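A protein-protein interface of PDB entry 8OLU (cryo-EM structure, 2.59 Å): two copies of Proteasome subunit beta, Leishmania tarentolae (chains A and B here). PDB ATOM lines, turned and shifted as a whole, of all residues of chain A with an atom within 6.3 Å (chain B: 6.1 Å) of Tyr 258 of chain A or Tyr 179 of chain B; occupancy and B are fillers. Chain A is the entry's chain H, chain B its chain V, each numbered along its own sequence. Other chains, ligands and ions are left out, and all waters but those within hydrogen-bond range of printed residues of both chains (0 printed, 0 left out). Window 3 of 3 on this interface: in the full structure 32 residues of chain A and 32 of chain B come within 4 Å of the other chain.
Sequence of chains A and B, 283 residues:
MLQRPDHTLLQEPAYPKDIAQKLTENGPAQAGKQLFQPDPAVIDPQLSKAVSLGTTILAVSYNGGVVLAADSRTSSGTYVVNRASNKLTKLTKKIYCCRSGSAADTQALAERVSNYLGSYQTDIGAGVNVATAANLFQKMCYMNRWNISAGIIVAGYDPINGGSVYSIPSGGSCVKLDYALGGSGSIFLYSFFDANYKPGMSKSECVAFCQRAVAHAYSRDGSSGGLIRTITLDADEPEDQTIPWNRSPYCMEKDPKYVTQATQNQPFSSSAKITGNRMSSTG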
ATOM      1  N   ARG A 220       2.809  21.798  12.883  1.00  0.00           N
ATOM      2  CA  ARG A 220       3.431  20.750  13.618  1.00  0.00           C
ATOM      3  C   ARG A 220       2.900  20.624  15.027  1.00  0.00           C
ATOM      4  O   ARG A 220       2.980  19.553  15.568  1.00  0.00           O
ATOM      5  CB  ARG A 220       4.924  21.061  13.649  1.00  0.00           C
ATOM      6  CG  ARG A 220       5.634  20.912  12.298  1.00  0.00           C
ATOM      7  CD  ARG A 220       5.721  19.479  11.925  1.00  0.00           C
ATOM      8  NE  ARG A 220       6.606  19.190  10.825  1.00  0.00           N
ATOM      9  CZ  ARG A 220       6.754  17.965  10.338  1.00  0.00           C
ATOM     10  NH1 ARG A 220       6.332  16.883  10.957  1.00  0.00           N
ATOM     11  NH2 ARG A 220       7.265  17.859   9.143  1.00  0.00           N
ATOM     12  N   TYR A 250       1.322  28.350   4.933  1.00  0.00           N
ATOM     13  CA  TYR A 250       1.991  27.068   4.883  1.00  0.00           C
ATOM     14  C   TYR A 250       1.117  26.012   5.509  1.00  0.00           C
ATOM     15  O   TYR A 250       0.533  26.231   6.550  1.00  0.00           O
ATOM     16  CB  TYR A 250       3.344  27.075   5.614  1.00  0.00           C
ATOM     17  CG  TYR A 250       4.042  25.733   5.580  1.00  0.00           C
ATOM     18  CD1 TYR A 250       4.615  25.254   4.425  1.00  0.00           C
ATOM     19  CD2 TYR A 250       3.976  24.862   6.655  1.00  0.00           C
ATOM     20  CE1 TYR A 250       5.222  24.013   4.358  1.00  0.00           C
ATOM     21  CE2 TYR A 250       4.494  23.576   6.567  1.00  0.00           C
ATOM     22  CZ  TYR A 250       5.140  23.150   5.420  1.00  0.00           C
ATOM     23  OH  TYR A 250       5.707  21.916   5.410  1.00  0.00           O
ATOM     24  N   CYS A 251       1.071  24.836   4.890  1.00  0.00           N
ATOM     25  CA  CYS A 251       0.750  23.642   5.662  1.00  0.00           C
ATOM     26  C   CYS A 251       1.344  22.403   5.022  1.00  0.00           C
ATOM     27  O   CYS A 251       1.525  22.378   3.810  1.00  0.00           O
ATOM     28  CB  CYS A 251      -0.759  23.476   5.753  1.00  0.00           C
ATOM     29  SG  CYS A 251      -1.534  23.282   4.139  1.00  0.00           S
ATOM     30  N   MET A 252       1.559  21.381   5.844  1.00  0.00           N
ATOM     31  CA  MET A 252       2.098  20.104   5.404  1.00  0.00           C
ATOM     32  C   MET A 252       1.198  19.430   4.390  1.00  0.00           C
ATOM     33  O   MET A 252       1.677  18.769   3.486  1.00  0.00           O
ATOM     34  CB  MET A 252       2.284  19.176   6.608  1.00  0.00           C
ATOM     35  CG  MET A 252       3.448  19.696   7.429  1.00  0.00           C
ATOM     36  SD  MET A 252       4.017  18.588   8.724  1.00  0.00           S
ATOM     37  CE  MET A 252       2.482  17.867   9.345  1.00  0.00           C
ATOM     38  N   GLU A 253      -0.094  19.623   4.494  1.00  0.00           N
ATOM     39  CA  GLU A 253      -1.023  18.983   3.591  1.00  0.00           C
ATOM     40  C   GLU A 253      -0.933  19.593   2.186  1.00  0.00           C
ATOM     41  O   GLU A 253      -1.722  19.244   1.319  1.00  0.00           O
ATOM     42  CB  GLU A 253      -2.458  19.182   4.118  1.00  0.00           C
ATOM     43  CG  GLU A 253      -2.729  18.826   5.608  1.00  0.00           C
ATOM     44  CD  GLU A 253      -2.638  19.831   6.782  1.00  0.00           C
ATOM     45  OE1 GLU A 253      -1.514  20.449   6.974  1.00  0.00           O
ATOM     46  OE2 GLU A 253      -3.623  19.898   7.633  1.00  0.00           O
ATOM     47  N   ASP A 255       2.378  21.165   1.132  1.00  0.00           N
ATOM     48  CA  ASP A 255       3.791  21.200   0.831  1.00  0.00           C
ATOM     49  C   ASP A 255       4.069  20.069  -0.149  1.00  0.00           C
ATOM     50  O   ASP A 255       3.738  18.924   0.143  1.00  0.00           O
ATOM     51  CB  ASP A 255       4.601  21.042   2.120  1.00  0.00           C
ATOM     52  CG  ASP A 255       6.104  21.316   1.997  1.00  0.00           C
ATOM     53  OD1 ASP A 255       6.603  21.362   0.825  1.00  0.00           O
ATOM     54  OD2 ASP A 255       6.790  21.510   3.072  1.00  0.00           O
ATOM     55  N   PRO A 256       4.678  20.308  -1.321  1.00  0.00           N
ATOM     56  CA  PRO A 256       4.929  19.213  -2.260  1.00  0.00           C
ATOM     57  C   PRO A 256       5.906  18.154  -1.779  1.00  0.00           C
ATOM     58  O   PRO A 256       5.829  16.997  -2.188  1.00  0.00           O
ATOM     59  CB  PRO A 256       5.490  19.902  -3.491  1.00  0.00           C
ATOM     60  CG  PRO A 256       5.086  21.396  -3.291  1.00  0.00           C
ATOM     61  CD  PRO A 256       5.121  21.626  -1.804  1.00  0.00           C
ATOM     62  N   LYS A 257       6.727  18.478  -0.796  1.00  0.00           N
ATOM     63  CA  LYS A 257       7.617  17.444  -0.318  1.00  0.00           C
ATOM     64  C   LYS A 257       6.977  16.466   0.650  1.00  0.00           C
ATOM     65  O   LYS A 257       7.693  15.645   1.189  1.00  0.00           O
ATOM     66  CB  LYS A 257       8.836  18.053   0.355  1.00  0.00           C
ATOM     67  CG  LYS A 257       8.599  18.649   1.724  1.00  0.00           C
ATOM     68  CD  LYS A 257       9.877  19.073   2.420  1.00  0.00           C
ATOM     69  CE  LYS A 257       9.608  20.080   3.526  1.00  0.00           C
ATOM     70  NZ  LYS A 257       9.501  21.450   2.977  1.00  0.00           N
ATOM     71  N   TYR A 258       5.675  16.569   0.917  1.00  0.00           N
ATOM     72  CA  TYR A 258       4.989  15.615   1.777  1.00  0.00           C
ATOM     73  C   TYR A 258       3.829  14.991   1.034  1.00  0.00           C
ATOM     74  O   TYR A 258       2.933  14.445   1.668  1.00  0.00           O
ATOM     75  CB  TYR A 258       4.463  16.274   3.070  1.00  0.00           C
ATOM     76  CG  TYR A 258       5.541  16.794   3.982  1.00  0.00           C
ATOM     77  CD1 TYR A 258       6.547  15.955   4.430  1.00  0.00           C
ATOM     78  CD2 TYR A 258       5.586  18.123   4.350  1.00  0.00           C
ATOM     79  CE1 TYR A 258       7.595  16.438   5.206  1.00  0.00           C
ATOM     80  CE2 TYR A 258       6.642  18.636   5.104  1.00  0.00           C
ATOM     81  CZ  TYR A 258       7.660  17.793   5.544  1.00  0.00           C
ATOM     82  OH  TYR A 258       8.715  18.269   6.302  1.00  0.00           O
ATOM     83  N   VAL A 259       3.840  15.091  -0.293  1.00  0.00           N
ATOM     84  CA  VAL A 259       2.827  14.477  -1.128  1.00  0.00           C
ATOM     85  C   VAL A 259       3.117  13.001  -1.366  1.00  0.00           C
ATOM     86  O   VAL A 259       2.183  12.200  -1.475  1.00  0.00           O
ATOM     87  CB  VAL A 259       2.748  15.169  -2.491  1.00  0.00           C
ATOM     88  CG1 VAL A 259       1.856  14.407  -3.440  1.00  0.00           C
ATOM     89  CG2 VAL A 259       2.258  16.590  -2.353  1.00  0.00           C
ATOM     90  N   THR A 260       4.375  12.622  -1.547  1.00  0.00           N
ATOM     91  CA  THR A 260       4.634  11.215  -1.727  1.00  0.00           C
ATOM     92  C   THR A 260       4.447  10.461  -0.412  1.00  0.00           C
ATOM     93  O   THR A 260       4.987  10.838   0.611  1.00  0.00           O
ATOM     94  CB  THR A 260       6.003  10.944  -2.355  1.00  0.00           C
ATOM     95  OG1 THR A 260       5.906  11.209  -3.761  1.00  0.00           O
ATOM     96  CG2 THR A 260       6.399   9.491  -2.201  1.00  0.00           C
ATOM     97  N   GLN A 261       3.697   9.349  -0.445  1.00  0.00           N
ATOM     98  CA  GLN A 261       3.494   8.636   0.795  1.00  0.00           C
ATOM     99  C   GLN A 261       4.728   7.824   1.127  1.00  0.00           C
ATOM    100  O   GLN A 261       5.360   7.228   0.265  1.00  0.00           O
ATOM    101  CB  GLN A 261       2.237   7.781   0.739  1.00  0.00           C
ATOM    102  CG  GLN A 261       0.969   8.612   0.830  1.00  0.00           C
ATOM    103  CD  GLN A 261      -0.205   7.845   1.370  1.00  0.00           C
ATOM    104  OE1 GLN A 261      -0.789   7.014   0.684  1.00  0.00           O
ATOM    105  NE2 GLN A 261      -0.568   8.123   2.608  1.00  0.00           N
ATOM    106  N   ALA B  59      18.854  12.367   9.332  1.00  0.00           N
ATOM    107  CA  ALA B  59      19.332  11.822   8.100  1.00  0.00           C
ATOM    108  C   ALA B  59      18.466  12.273   6.986  1.00  0.00           C
ATOM    109  O   ALA B  59      17.289  12.244   7.140  1.00  0.00           O
ATOM    110  CB  ALA B  59      19.349  10.313   8.132  1.00  0.00           C
ATOM    111  N   VAL B  60      19.087  12.435   5.858  1.00  0.00           N
ATOM    112  CA  VAL B  60      18.460  12.946   4.680  1.00  0.00           C
ATOM    113  C   VAL B  60      18.916  12.154   3.471  1.00  0.00           C
ATOM    114  O   VAL B  60      20.037  11.728   3.343  1.00  0.00           O
ATOM    115  CB  VAL B  60      18.858  14.420   4.541  1.00  0.00           C
ATOM    116  CG1 VAL B  60      18.136  15.026   3.374  1.00  0.00           C
ATOM    117  CG2 VAL B  60      18.539  15.230   5.791  1.00  0.00           C
ATOM    118  N   SER B  61      18.002  11.957   2.568  1.00  0.00           N
ATOM    119  CA  SER B  61      18.263  11.286   1.316  1.00  0.00           C
ATOM    120  C   SER B  61      18.673  12.311   0.286  1.00  0.00           C
ATOM    121  O   SER B  61      18.304  13.469   0.375  1.00  0.00           O
ATOM    122  CB  SER B  61      17.001  10.605   0.896  1.00  0.00           C
ATOM    123  OG  SER B  61      16.597   9.606   1.844  1.00  0.00           O
ATOM    124  N   VAL B 165      16.337   5.740   4.469  1.00  0.00           N
ATOM    125  CA  VAL B 165      16.309   6.290   5.803  1.00  0.00           C
ATOM    126  C   VAL B 165      15.147   5.693   6.512  1.00  0.00           C
ATOM    127  O   VAL B 165      14.033   5.798   6.060  1.00  0.00           O
ATOM    128  CB  VAL B 165      16.138   7.802   5.717  1.00  0.00           C
ATOM    129  CG1 VAL B 165      16.052   8.472   7.055  1.00  0.00           C
ATOM    130  CG2 VAL B 165      17.301   8.381   5.005  1.00  0.00           C
ATOM    131  N   LEU B 177      11.394   7.013   5.335  1.00  0.00           N
ATOM    132  CA  LEU B 177      11.155   8.381   4.999  1.00  0.00           C
ATOM    133  C   LEU B 177      12.186   8.895   4.058  1.00  0.00           C
ATOM    134  O   LEU B 177      13.176   8.257   3.836  1.00  0.00           O
ATOM    135  CB  LEU B 177      11.358   9.117   6.299  1.00  0.00           C
ATOM    136  CG  LEU B 177      10.321   8.756   7.329  1.00  0.00           C
ATOM    137  CD1 LEU B 177      10.893   9.126   8.704  1.00  0.00           C
ATOM    138  CD2 LEU B 177       8.996   9.423   6.970  1.00  0.00           C
ATOM    139  N   ASP B 178      11.963  10.114   3.657  1.00  0.00           N
ATOM    140  CA  ASP B 178      12.934  10.849   2.911  1.00  0.00           C
ATOM    141  C   ASP B 178      14.009  11.433   3.821  1.00  0.00           C
ATOM    142  O   ASP B 178      15.171  11.553   3.451  1.00  0.00           O
ATOM    143  CB  ASP B 178      12.227  11.992   2.216  1.00  0.00           C
ATOM    144  CG  ASP B 178      13.156  12.584   1.182  1.00  0.00           C
ATOM    145  OD1 ASP B 178      13.606  11.758   0.299  1.00  0.00           O
ATOM    146  OD2 ASP B 178      13.475  13.825   1.279  1.00  0.00           O
ATOM    147  N   TYR B 179      13.575  11.932   4.957  1.00  0.00           N
ATOM    148  CA  TYR B 179      14.509  12.341   5.946  1.00  0.00           C
ATOM    149  C   TYR B 179      13.931  12.043   7.299  1.00  0.00           C
ATOM    150  O   TYR B 179      12.752  11.939   7.422  1.00  0.00           O
ATOM    151  CB  TYR B 179      14.776  13.839   5.795  1.00  0.00           C
ATOM    152  CG  TYR B 179      13.636  14.731   6.178  1.00  0.00           C
ATOM    153  CD1 TYR B 179      13.353  14.968   7.504  1.00  0.00           C
ATOM    154  CD2 TYR B 179      12.773  15.220   5.237  1.00  0.00           C
ATOM    155  CE1 TYR B 179      12.268  15.746   7.891  1.00  0.00           C
ATOM    156  CE2 TYR B 179      11.683  15.999   5.596  1.00  0.00           C
ATOM    157  CZ  TYR B 179      11.416  16.251   6.930  1.00  0.00           C
ATOM    158  OH  TYR B 179      10.363  17.012   7.363  1.00  0.00           O
ATOM    159  N   ALA B 180      14.763  12.040   8.311  1.00  0.00           N
ATOM    160  CA  ALA B 180      14.311  11.752   9.636  1.00  0.00           C
ATOM    161  C   ALA B 180      15.104  12.536  10.622  1.00  0.00           C
ATOM    162  O   ALA B 180      16.228  12.803  10.398  1.00  0.00           O
ATOM    163  CB  ALA B 180      14.495  10.302   9.896  1.00  0.00           C
ATOM    164  N   LEU B 181      14.489  12.833  11.725  1.00  0.00           N
ATOM    165  CA  LEU B 181      15.018  13.634  12.794  1.00  0.00           C
ATOM    166  C   LEU B 181      14.820  12.887  14.065  1.00  0.00           C
ATOM    167  O   LEU B 181      13.864  12.171  14.190  1.00  0.00           O
ATOM    168  CB  LEU B 181      14.172  14.869  12.911  1.00  0.00           C
ATOM    169  CG  LEU B 181      13.938  15.565  11.594  1.00  0.00           C
ATOM    170  CD1 LEU B 181      13.063  16.761  11.861  1.00  0.00           C
ATOM    171  CD2 LEU B 181      15.229  16.067  11.025  1.00  0.00           C
ATOM    172  N   TYR B 190      11.864  20.516  12.871  1.00  0.00           N
ATOM    173  CA  TYR B 190      10.698  20.274  12.070  1.00  0.00           C
ATOM    174  C   TYR B 190      10.329  21.477  11.243  1.00  0.00           C
ATOM    175  O   TYR B 190      10.271  21.411  10.052  1.00  0.00           O
ATOM    176  CB  TYR B 190       9.589  19.845  13.001  1.00  0.00           C
ATOM    177  CG  TYR B 190       9.748  18.411  13.368  1.00  0.00           C
ATOM    178  CD1 TYR B 190       9.727  17.461  12.371  1.00  0.00           C
ATOM    179  CD2 TYR B 190       9.980  18.016  14.672  1.00  0.00           C
ATOM    180  CE1 TYR B 190       9.873  16.113  12.662  1.00  0.00           C
ATOM    181  CE2 TYR B 190      10.153  16.662  14.969  1.00  0.00           C
ATOM    182  CZ  TYR B 190      10.115  15.708  13.954  1.00  0.00           C
ATOM    183  OH  TYR B 190      10.305  14.339  14.208  1.00  0.00           O
ATOM    184  N   PHE B 193      12.966  22.196   8.512  1.00  0.00           N
ATOM    185  CA  PHE B 193      12.806  21.404   7.327  1.00  0.00           C
ATOM    186  C   PHE B 193      11.575  21.794   6.527  1.00  0.00           C
ATOM    187  O   PHE B 193      11.625  21.909   5.302  1.00  0.00           O
ATOM    188  CB  PHE B 193      12.724  19.960   7.765  1.00  0.00           C
ATOM    189  CG  PHE B 193      14.088  19.364   7.865  1.00  0.00           C
ATOM    190  CD1 PHE B 193      14.890  19.637   8.939  1.00  0.00           C
ATOM    191  CD2 PHE B 193      14.556  18.515   6.867  1.00  0.00           C
ATOM    192  CE1 PHE B 193      16.164  19.127   8.994  1.00  0.00           C
ATOM    193  CE2 PHE B 193      15.853  18.025   6.912  1.00  0.00           C
ATOM    194  CZ  PHE B 193      16.653  18.360   7.973  1.00  0.00           C
ATOM    195  N   ASP B 194      10.446  21.868   7.203  1.00  0.00           N
ATOM    196  CA  ASP B 194       9.238  22.346   6.576  1.00  0.00           C
ATOM    197  C   ASP B 194       9.540  23.618   5.801  1.00  0.00           C
ATOM    198  O   ASP B 194       9.181  23.777   4.649  1.00  0.00           O
ATOM    199  CB  ASP B 194       8.176  22.581   7.631  1.00  0.00           C
ATOM    200  CG  ASP B 194       7.549  21.331   8.256  1.00  0.00           C
ATOM    201  OD1 ASP B 194       8.011  20.184   7.959  1.00  0.00           O
ATOM    202  OD2 ASP B 194       6.635  21.501   9.130  1.00  0.00           O
ATOM    203  N   TYR B 197      14.014  22.954   3.799  1.00  0.00           N
ATOM    204  CA  TYR B 197      14.475  21.779   3.088  1.00  0.00           C
ATOM    205  C   TYR B 197      13.728  21.543   1.806  1.00  0.00           C
ATOM    206  O   TYR B 197      12.566  21.222   1.839  1.00  0.00           O
ATOM    207  CB  TYR B 197      14.211  20.547   3.942  1.00  0.00           C
ATOM    208  CG  TYR B 197      14.520  19.239   3.281  1.00  0.00           C
ATOM    209  CD1 TYR B 197      15.817  18.841   3.042  1.00  0.00           C
ATOM    210  CD2 TYR B 197      13.489  18.372   2.953  1.00  0.00           C
ATOM    211  CE1 TYR B 197      16.081  17.631   2.423  1.00  0.00           C
ATOM    212  CE2 TYR B 197      13.732  17.120   2.408  1.00  0.00           C
ATOM    213  CZ  TYR B 197      15.046  16.752   2.138  1.00  0.00           C
ATOM    214  OH  TYR B 197      15.235  15.511   1.553  1.00  0.00           O
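No position is printed for both chains. Of the 11 pairs that touch across the chains among the printed residues, none has its exchanged pair printed and touching as well.
NH2 of Arg 220 of chain A lies close to SD of Met 252 of chain A. The guanidinium group (NH2) of Arg 220 of chain A is in hydrogen-bond range of the side-chain hydroxyl (OH) of Tyr 258 of chain A, 3.2 Å away. The side-chain hydroxyl (OH) of Tyr 250 of chain A is in hydrogen-bond range of the side-chain carboxylate (OD2) of Asp 255 of chain A (2.6 Å). NZ of Lys 257 of chain A is in salt-bridge range of OD2 of Asp 255 of chain A, at 2.7 Å. OD2 of Asp 178 of chain B sits at hydrogen-bond distance from OH of Tyr 197 of chain B (2.5 Å).
Of the printed residues of chain B, Asp 255 of chain A touches Asp 194. Tyr 258 of chain A touches two residues of chain B. Gln 261 of chain A touches none of the printed residues of chain B. Ala 59 of chain B touches none of the printed residues of chain A. Of the printed residues of chain A, Tyr 190 of chain B touches Arg 220 (3.6 Å). Printed residues of chain A within 4 Å of Phe 193 of chain B: Lys 257. Printed residues of chain A within 4 Å of Asp 194 of chain B: Arg 220, Tyr 250, Met 252, Asp 255, Lys 257 and Tyr 258.
The side-chain carboxylate (OD1) of Asp 194 of chain B lies within salt-bridge range of the guanidinium group (NH2) of Arg 220 of chain A (2.7 Å). NZ of Lys 257 of chain A is in hydrogen-bond range of O of Phe 193 of chain B (3.2 Å). The side-chain amino group (NZ) of Lys 257 of chain A sits at hydrogen-bond distance from the backbone carbonyl oxygen (O) of Asp 194 of chain B, at 2.9 Å. NZ of Lys 257 of chain A lies within hydrogen-bond range of O of Tyr 197 of chain B, at 3.3 Å. OH of Tyr 258 of chain A sits at hydrogen-bond distance from OD1 of Asp 194 of chain B (2.6 Å). The side-chain hydroxyl (OH) of Tyr 258 of chain A lies close to the side-chain hydroxyl (OH) of Tyr 179 of chain B, at 2.3 Å.
Among the printed residues, pairs that only touch across the chains: Arg 220 of chain A with Tyr 179 of chain B, Arg 220 of chain A with Tyr 190 of chain B, Tyr 250 of chain A with Asp 194 of chain B, Met 252 of chain A with Asp 194 of chain B and Asp 255 of chain A with Asp 194 of chain B.
Of the 12 printed residues of chain A, 6 touch a printed residue of chain B. Hydrophobic or aromatic side chains of chain B that line the printed part of chain A: Tyr 179, Tyr 190 and Tyr 197. Among the printed residues, Asp or Glu carboxylates within 4 Å of a Lys or Arg side-chain nitrogen of the other chain: Arg 220 of chain A with Asp 194 of chain B.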
